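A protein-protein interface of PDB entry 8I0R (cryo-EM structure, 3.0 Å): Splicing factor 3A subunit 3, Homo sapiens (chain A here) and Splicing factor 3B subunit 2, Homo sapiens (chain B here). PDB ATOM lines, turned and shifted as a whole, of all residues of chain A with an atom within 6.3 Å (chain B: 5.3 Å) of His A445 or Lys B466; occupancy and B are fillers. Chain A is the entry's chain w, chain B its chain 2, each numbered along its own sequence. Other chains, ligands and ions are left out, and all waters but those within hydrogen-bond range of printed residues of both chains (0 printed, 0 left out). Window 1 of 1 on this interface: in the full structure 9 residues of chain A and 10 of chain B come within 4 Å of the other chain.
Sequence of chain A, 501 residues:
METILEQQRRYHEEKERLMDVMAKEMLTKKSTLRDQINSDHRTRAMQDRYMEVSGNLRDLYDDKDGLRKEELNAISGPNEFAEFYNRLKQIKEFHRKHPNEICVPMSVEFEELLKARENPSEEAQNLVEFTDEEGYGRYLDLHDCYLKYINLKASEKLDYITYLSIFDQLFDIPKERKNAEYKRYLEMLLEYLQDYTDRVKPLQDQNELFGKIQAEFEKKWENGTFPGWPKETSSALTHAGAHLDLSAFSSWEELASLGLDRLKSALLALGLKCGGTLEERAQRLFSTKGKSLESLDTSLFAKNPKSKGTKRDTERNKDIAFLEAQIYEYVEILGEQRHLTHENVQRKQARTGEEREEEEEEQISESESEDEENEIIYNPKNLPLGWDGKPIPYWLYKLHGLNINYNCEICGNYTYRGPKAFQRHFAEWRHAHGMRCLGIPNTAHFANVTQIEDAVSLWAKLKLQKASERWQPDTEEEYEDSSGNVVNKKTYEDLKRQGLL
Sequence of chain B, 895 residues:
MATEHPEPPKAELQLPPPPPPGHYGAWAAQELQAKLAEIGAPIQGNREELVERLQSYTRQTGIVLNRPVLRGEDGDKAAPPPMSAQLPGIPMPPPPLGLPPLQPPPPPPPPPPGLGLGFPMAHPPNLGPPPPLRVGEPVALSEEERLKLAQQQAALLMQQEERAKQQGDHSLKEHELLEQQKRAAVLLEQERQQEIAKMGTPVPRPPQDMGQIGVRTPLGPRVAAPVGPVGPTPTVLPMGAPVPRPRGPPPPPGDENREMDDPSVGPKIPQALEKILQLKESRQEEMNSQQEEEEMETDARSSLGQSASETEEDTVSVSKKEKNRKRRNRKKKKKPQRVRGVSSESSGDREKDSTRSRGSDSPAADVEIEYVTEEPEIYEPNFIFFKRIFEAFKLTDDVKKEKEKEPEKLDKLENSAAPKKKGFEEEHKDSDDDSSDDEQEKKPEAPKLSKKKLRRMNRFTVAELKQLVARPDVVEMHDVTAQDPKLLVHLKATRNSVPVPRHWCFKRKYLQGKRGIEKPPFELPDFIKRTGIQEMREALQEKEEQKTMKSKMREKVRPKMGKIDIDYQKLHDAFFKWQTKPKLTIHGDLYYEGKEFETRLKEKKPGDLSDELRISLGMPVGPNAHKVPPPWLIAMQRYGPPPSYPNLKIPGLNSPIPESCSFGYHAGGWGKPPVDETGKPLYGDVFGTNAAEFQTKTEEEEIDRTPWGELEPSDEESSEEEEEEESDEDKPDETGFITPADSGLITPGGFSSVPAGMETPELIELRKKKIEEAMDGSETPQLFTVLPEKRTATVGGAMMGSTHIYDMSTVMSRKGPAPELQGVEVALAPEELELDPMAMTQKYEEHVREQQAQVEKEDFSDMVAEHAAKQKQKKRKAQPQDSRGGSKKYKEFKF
Among the printed residues, pairs that only touch across the chains: Leu A458 with Lys B466 (3.3 Å), Lys A461 with Lys B466 (3.6 Å), Asn A448 with Val B462 (3.6 Å), His A445 with Pro B472 (3.7 Å), His A445 with Asp B473 (3.7 Å) and Leu A458 with Gln B467 (3.9 Å).
His A445 touches three residues of chain B.
Of the printed residues of chain B, Asn A448 touches Val B462.
Printed residues of chain B within 4 Å of Leu A458: Lys B466 and Gln B467.
Printed residues of chain A within 4 Å of Val B462: Asn A448.
Lys B466 touches just these residues of chain A: His A445, Ala A447, Leu A458 and Lys A461.
Printed residues of chain A within 4 Å of Gln B467: Leu A458 and Lys A461.
The nearest residue of chain A that does not touch Lys B466 is Ala A444 (4.04 Å).
The nearest printed residue of chain A that does not touch Asp B473 is Ala A444 (4.5 Å).
Hydrophobic or aromatic side chains of chain A that line the printed part of chain B: His A445 and Leu A458.
Of the 12 printed residues of chain B, 6 touch a printed residue of chain A.
Along chain B the printed residues that touch a printed residue of chain A span positions 462 to 473.
Among the printed residues, 10 pairs touch across the chains.
Among the printed residues, no Asp or Glu carboxylate lies within 4 Å of a Lys or Arg side-chain nitrogen of the other chain.
NZ of Lys B466 sits at hydrogen-bond distance from O of His A445.
NZ of Lys A461 lies within hydrogen-bond range of O of Val B469.
NZ of Lys B466 sits at hydrogen-bond distance from O of Ala A447.
The side-chain amino group (NZ) of Lys A461 sits at hydrogen-bond distance from the backbone carbonyl oxygen (O) of Gln B467.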
ATOM      1  N   THR A 443      37.279  -7.749   8.527  1.00  0.00           N
ATOM      2  CA  THR A 443      36.838  -8.852   9.360  1.00  0.00           C
ATOM      3  C   THR A 443      35.976  -9.787   8.533  1.00  0.00           C
ATOM      4  O   THR A 443      35.714  -9.551   7.352  1.00  0.00           O
ATOM      5  CB  THR A 443      36.044  -8.366  10.568  1.00  0.00           C
ATOM      6  OG1 THR A 443      35.988  -6.934  10.555  1.00  0.00           O
ATOM      7  CG2 THR A 443      36.688  -8.836  11.850  1.00  0.00           C
ATOM      8  N   ALA A 444      35.523 -10.856   9.181  1.00  0.00           N
ATOM      9  CA  ALA A 444      34.752 -11.872   8.485  1.00  0.00           C
ATOM     10  C   ALA A 444      33.484 -11.311   7.862  1.00  0.00           C
ATOM     11  O   ALA A 444      33.120 -11.715   6.753  1.00  0.00           O
ATOM     12  CB  ALA A 444      34.407 -13.005   9.451  1.00  0.00           C
ATOM     13  N   HIS A 445      32.824 -10.372   8.538  1.00  0.00           N
ATOM     14  CA  HIS A 445      31.449 -10.032   8.196  1.00  0.00           C
ATOM     15  C   HIS A 445      31.335  -9.434   6.804  1.00  0.00           C
ATOM     16  O   HIS A 445      30.277  -9.525   6.175  1.00  0.00           O
ATOM     17  CB  HIS A 445      30.885  -9.062   9.225  1.00  0.00           C
ATOM     18  CG  HIS A 445      31.033  -9.524  10.639  1.00  0.00           C
ATOM     19  ND1 HIS A 445      30.008  -9.445  11.553  1.00  0.00           N
ATOM     20  CD2 HIS A 445      32.094 -10.034  11.307  1.00  0.00           C
ATOM     21  CE1 HIS A 445      30.424  -9.908  12.718  1.00  0.00           C
ATOM     22  NE2 HIS A 445      31.688 -10.269  12.596  1.00  0.00           N
ATOM     23  N   PHE A 446      32.405  -8.824   6.305  1.00  0.00           N
ATOM     24  CA  PHE A 446      32.384  -8.091   5.050  1.00  0.00           C
ATOM     25  C   PHE A 446      32.946  -8.889   3.889  1.00  0.00           C
ATOM     26  O   PHE A 446      32.950  -8.397   2.757  1.00  0.00           O
ATOM     27  CB  PHE A 446      33.136  -6.781   5.222  1.00  0.00           C
ATOM     28  CG  PHE A 446      32.741  -6.047   6.453  1.00  0.00           C
ATOM     29  CD1 PHE A 446      31.625  -5.237   6.453  1.00  0.00           C
ATOM     30  CD2 PHE A 446      33.449  -6.200   7.620  1.00  0.00           C
ATOM     31  CE1 PHE A 446      31.243  -4.566   7.578  1.00  0.00           C
ATOM     32  CE2 PHE A 446      33.065  -5.542   8.751  1.00  0.00           C
ATOM     33  CZ  PHE A 446      31.958  -4.722   8.729  1.00  0.00           C
ATOM     34  N   ALA A 447      33.417 -10.103   4.143  1.00  0.00           N
ATOM     35  CA  ALA A 447      33.841 -10.971   3.061  1.00  0.00           C
ATOM     36  C   ALA A 447      32.686 -11.212   2.103  1.00  0.00           C
ATOM     37  O   ALA A 447      31.551 -11.433   2.528  1.00  0.00           O
ATOM     38  CB  ALA A 447      34.357 -12.289   3.620  1.00  0.00           C
ATOM     39  N   ASN A 448      32.986 -11.145   0.807  1.00  0.00           N
ATOM     40  CA  ASN A 448      32.069 -11.292  -0.322  1.00  0.00           C
ATOM     41  C   ASN A 448      31.221 -10.055  -0.551  1.00  0.00           C
ATOM     42  O   ASN A 448      30.372 -10.057  -1.445  1.00  0.00           O
ATOM     43  CB  ASN A 448      31.177 -12.526  -0.193  1.00  0.00           C
ATOM     44  CG  ASN A 448      31.945 -13.803  -0.393  1.00  0.00           C
ATOM     45  OD1 ASN A 448      32.377 -14.105  -1.499  1.00  0.00           O
ATOM     46  ND2 ASN A 448      32.137 -14.555   0.679  1.00  0.00           N
ATOM     47  N   VAL A 449      31.435  -8.996   0.222  1.00  0.00           N
ATOM     48  CA  VAL A 449      30.939  -7.667  -0.112  1.00  0.00           C
ATOM     49  C   VAL A 449      32.024  -6.963  -0.917  1.00  0.00           C
ATOM     50  O   VAL A 449      33.188  -6.940  -0.518  1.00  0.00           O
ATOM     51  CB  VAL A 449      30.576  -6.877   1.149  1.00  0.00           C
ATOM     52  CG1 VAL A 449      30.446  -5.403   0.837  1.00  0.00           C
ATOM     53  CG2 VAL A 449      29.282  -7.401   1.719  1.00  0.00           C
ATOM     54  N   LEU A 458      26.457  -1.655   5.663  1.00  0.00           N
ATOM     55  CA  LEU A 458      26.563  -2.817   6.533  1.00  0.00           C
ATOM     56  C   LEU A 458      27.371  -2.499   7.777  1.00  0.00           C
ATOM     57  O   LEU A 458      27.005  -2.906   8.883  1.00  0.00           O
ATOM     58  CB  LEU A 458      27.201  -3.966   5.767  1.00  0.00           C
ATOM     59  CG  LEU A 458      27.160  -5.346   6.383  1.00  0.00           C
ATOM     60  CD1 LEU A 458      25.764  -5.887   6.236  1.00  0.00           C
ATOM     61  CD2 LEU A 458      28.156  -6.205   5.648  1.00  0.00           C
ATOM     62  N   LYS A 461      25.026  -0.687  10.207  1.00  0.00           N
ATOM     63  CA  LYS A 461      24.101  -1.516  10.972  1.00  0.00           C
ATOM     64  C   LYS A 461      24.859  -2.401  11.957  1.00  0.00           C
ATOM     65  O   LYS A 461      24.359  -2.703  13.043  1.00  0.00           O
ATOM     66  CB  LYS A 461      23.209  -2.347  10.053  1.00  0.00           C
ATOM     67  CG  LYS A 461      23.917  -3.364   9.219  1.00  0.00           C
ATOM     68  CD  LYS A 461      23.045  -4.591   9.065  1.00  0.00           C
ATOM     69  CE  LYS A 461      23.415  -5.676  10.053  1.00  0.00           C
ATOM     70  NZ  LYS A 461      22.753  -6.951   9.710  1.00  0.00           N
ATOM     71  N   LEU A 462      26.077  -2.806  11.613  1.00  0.00           N
ATOM     72  CA  LEU A 462      26.863  -3.613  12.538  1.00  0.00           C
ATOM     73  C   LEU A 462      27.350  -2.781  13.714  1.00  0.00           C
ATOM     74  O   LEU A 462      27.446  -3.279  14.844  1.00  0.00           O
ATOM     75  CB  LEU A 462      28.035  -4.241  11.796  1.00  0.00           C
ATOM     76  CG  LEU A 462      28.841  -5.380  12.413  1.00  0.00           C
ATOM     77  CD1 LEU A 462      29.516  -6.154  11.303  1.00  0.00           C
ATOM     78  CD2 LEU A 462      29.876  -4.893  13.404  1.00  0.00           C
ATOM     79  N   THR B 461      21.127 -10.025  -3.719  1.00  0.00           N
ATOM     80  CA  THR B 461      22.563  -9.880  -3.760  1.00  0.00           C
ATOM     81  C   THR B 461      23.136 -10.257  -2.404  1.00  0.00           C
ATOM     82  O   THR B 461      22.439 -10.258  -1.384  1.00  0.00           O
ATOM     83  CB  THR B 461      22.948  -8.448  -4.117  1.00  0.00           C
ATOM     84  OG1 THR B 461      22.938  -7.646  -2.932  1.00  0.00           O
ATOM     85  CG2 THR B 461      21.957  -7.874  -5.115  1.00  0.00           C
ATOM     86  N   VAL B 462      24.422 -10.598  -2.400  1.00  0.00           N
ATOM     87  CA  VAL B 462      25.023 -11.051  -1.158  1.00  0.00           C
ATOM     88  C   VAL B 462      24.948  -9.960  -0.108  1.00  0.00           C
ATOM     89  O   VAL B 462      24.785 -10.245   1.077  1.00  0.00           O
ATOM     90  CB  VAL B 462      26.464 -11.527  -1.399  1.00  0.00           C
ATOM     91  CG1 VAL B 462      27.286 -11.417  -0.138  1.00  0.00           C
ATOM     92  CG2 VAL B 462      26.456 -12.957  -1.864  1.00  0.00           C
ATOM     93  N   ALA B 463      24.995  -8.699  -0.517  1.00  0.00           N
ATOM     94  CA  ALA B 463      24.917  -7.631   0.469  1.00  0.00           C
ATOM     95  C   ALA B 463      23.484  -7.435   0.931  1.00  0.00           C
ATOM     96  O   ALA B 463      23.239  -7.098   2.092  1.00  0.00           O
ATOM     97  CB  ALA B 463      25.484  -6.341  -0.106  1.00  0.00           C
ATOM     98  N   GLU B 464      22.525  -7.665   0.038  1.00  0.00           N
ATOM     99  CA  GLU B 464      21.131  -7.755   0.455  1.00  0.00           C
ATOM    100  C   GLU B 464      20.970  -8.734   1.611  1.00  0.00           C
ATOM    101  O   GLU B 464      20.459  -8.376   2.684  1.00  0.00           O
ATOM    102  CB  GLU B 464      20.274  -8.184  -0.735  1.00  0.00           C
ATOM    103  CG  GLU B 464      18.843  -7.691  -0.742  1.00  0.00           C
ATOM    104  CD  GLU B 464      18.709  -6.204  -0.522  1.00  0.00           C
ATOM    105  OE1 GLU B 464      19.624  -5.454  -0.920  1.00  0.00           O
ATOM    106  OE2 GLU B 464      17.673  -5.781   0.035  1.00  0.00           O
ATOM    107  N   LEU B 465      21.406  -9.978   1.400  1.00  0.00           N
ATOM    108  CA  LEU B 465      21.365 -10.973   2.462  1.00  0.00           C
ATOM    109  C   LEU B 465      22.112 -10.494   3.696  1.00  0.00           C
ATOM    110  O   LEU B 465      21.510 -10.324   4.758  1.00  0.00           O
ATOM    111  CB  LEU B 465      21.944 -12.290   1.956  1.00  0.00           C
ATOM    112  CG  LEU B 465      21.368 -13.612   2.444  1.00  0.00           C
ATOM    113  CD1 LEU B 465      19.948 -13.432   2.890  1.00  0.00           C
ATOM    114  CD2 LEU B 465      21.416 -14.599   1.311  1.00  0.00           C
ATOM    115  N   LYS B 466      23.414 -10.238   3.566  1.00  0.00           N
ATOM    116  CA  LYS B 466      24.239  -9.827   4.697  1.00  0.00           C
ATOM    117  C   LYS B 466      23.607  -8.698   5.485  1.00  0.00           C
ATOM    118  O   LYS B 466      23.888  -8.546   6.676  1.00  0.00           O
ATOM    119  CB  LYS B 466      25.616  -9.395   4.209  1.00  0.00           C
ATOM    120  CG  LYS B 466      26.436 -10.488   3.591  1.00  0.00           C
ATOM    121  CD  LYS B 466      27.737 -10.661   4.317  1.00  0.00           C
ATOM    122  CE  LYS B 466      28.547 -11.778   3.708  1.00  0.00           C
ATOM    123  NZ  LYS B 466      29.794 -12.003   4.479  1.00  0.00           N
ATOM    124  N   GLN B 467      22.767  -7.893   4.842  1.00  0.00           N
ATOM    125  CA  GLN B 467      22.063  -6.818   5.518  1.00  0.00           C
ATOM    126  C   GLN B 467      20.902  -7.342   6.338  1.00  0.00           C
ATOM    127  O   GLN B 467      20.823  -7.088   7.542  1.00  0.00           O
ATOM    128  CB  GLN B 467      21.543  -5.803   4.508  1.00  0.00           C
ATOM    129  CG  GLN B 467      20.838  -4.642   5.154  1.00  0.00           C
ATOM    130  CD  GLN B 467      21.598  -3.356   4.984  1.00  0.00           C
ATOM    131  OE1 GLN B 467      21.047  -2.354   4.541  1.00  0.00           O
ATOM    132  NE2 GLN B 467      22.878  -3.378   5.324  1.00  0.00           N
ATOM    133  N   LEU B 468      19.985  -8.054   5.685  1.00  0.00           N
ATOM    134  CA  LEU B 468      18.748  -8.429   6.368  1.00  0.00           C
ATOM    135  C   LEU B 468      19.017  -9.306   7.583  1.00  0.00           C
ATOM    136  O   LEU B 468      18.542  -9.014   8.685  1.00  0.00           O
ATOM    137  CB  LEU B 468      17.800  -9.133   5.408  1.00  0.00           C
ATOM    138  CG  LEU B 468      17.639  -8.406   4.081  1.00  0.00           C
ATOM    139  CD1 LEU B 468      16.747  -9.187   3.131  1.00  0.00           C
ATOM    140  CD2 LEU B 468      17.093  -7.014   4.336  1.00  0.00           C
ATOM    141  N   VAL B 469      19.779 -10.382   7.401  1.00  0.00           N
ATOM    142  CA  VAL B 469      19.960 -11.374   8.451  1.00  0.00           C
ATOM    143  C   VAL B 469      20.639 -10.765   9.669  1.00  0.00           C
ATOM    144  O   VAL B 469      21.306  -9.729   9.582  1.00  0.00           O
ATOM    145  CB  VAL B 469      20.766 -12.551   7.889  1.00  0.00           C
ATOM    146  CG1 VAL B 469      20.706 -13.722   8.839  1.00  0.00           C
ATOM    147  CG2 VAL B 469      20.230 -12.927   6.541  1.00  0.00           C
ATOM    148  N   PRO B 472      25.746 -11.720   9.868  1.00  0.00           N
ATOM    149  CA  PRO B 472      26.150 -11.759   8.463  1.00  0.00           C
ATOM    150  C   PRO B 472      27.369 -12.622   8.207  1.00  0.00           C
ATOM    151  O   PRO B 472      27.535 -13.141   7.101  1.00  0.00           O
ATOM    152  CB  PRO B 472      26.438 -10.289   8.166  1.00  0.00           C
ATOM    153  CG  PRO B 472      27.007  -9.809   9.441  1.00  0.00           C
ATOM    154  CD  PRO B 472      26.258 -10.517  10.540  1.00  0.00           C
ATOM    155  N   ASP B 473      28.216 -12.793   9.220  1.00  0.00           N
ATOM    156  CA  ASP B 473      29.413 -13.608   9.059  1.00  0.00           C
ATOM    157  C   ASP B 473      29.060 -14.941   8.436  1.00  0.00           C
ATOM    158  O   ASP B 473      29.667 -15.380   7.456  1.00  0.00           O
ATOM    159  CB  ASP B 473      30.065 -13.824  10.417  1.00  0.00           C
ATOM    160  CG  ASP B 473      29.124 -13.514  11.552  1.00  0.00           C
ATOM    161  OD1 ASP B 473      27.939 -13.239  11.274  1.00  0.00           O
ATOM    162  OD2 ASP B 473      29.562 -13.533  12.720  1.00  0.00           O
ATOM    163  N   VAL B 475      26.848 -15.843   6.474  1.00  0.00           N
ATOM    164  CA  VAL B 475      26.464 -15.894   5.067  1.00  0.00           C
ATOM    165  C   VAL B 475      27.721 -16.112   4.236  1.00  0.00           C
ATOM    166  O   VAL B 475      28.695 -15.369   4.357  1.00  0.00           O
ATOM    167  CB  VAL B 475      25.733 -14.625   4.628  1.00  0.00           C
ATOM    168  CG1 VAL B 475      25.168 -14.812   3.242  1.00  0.00           C
ATOM    169  CG2 VAL B 475      24.651 -14.262   5.607  1.00  0.00           C
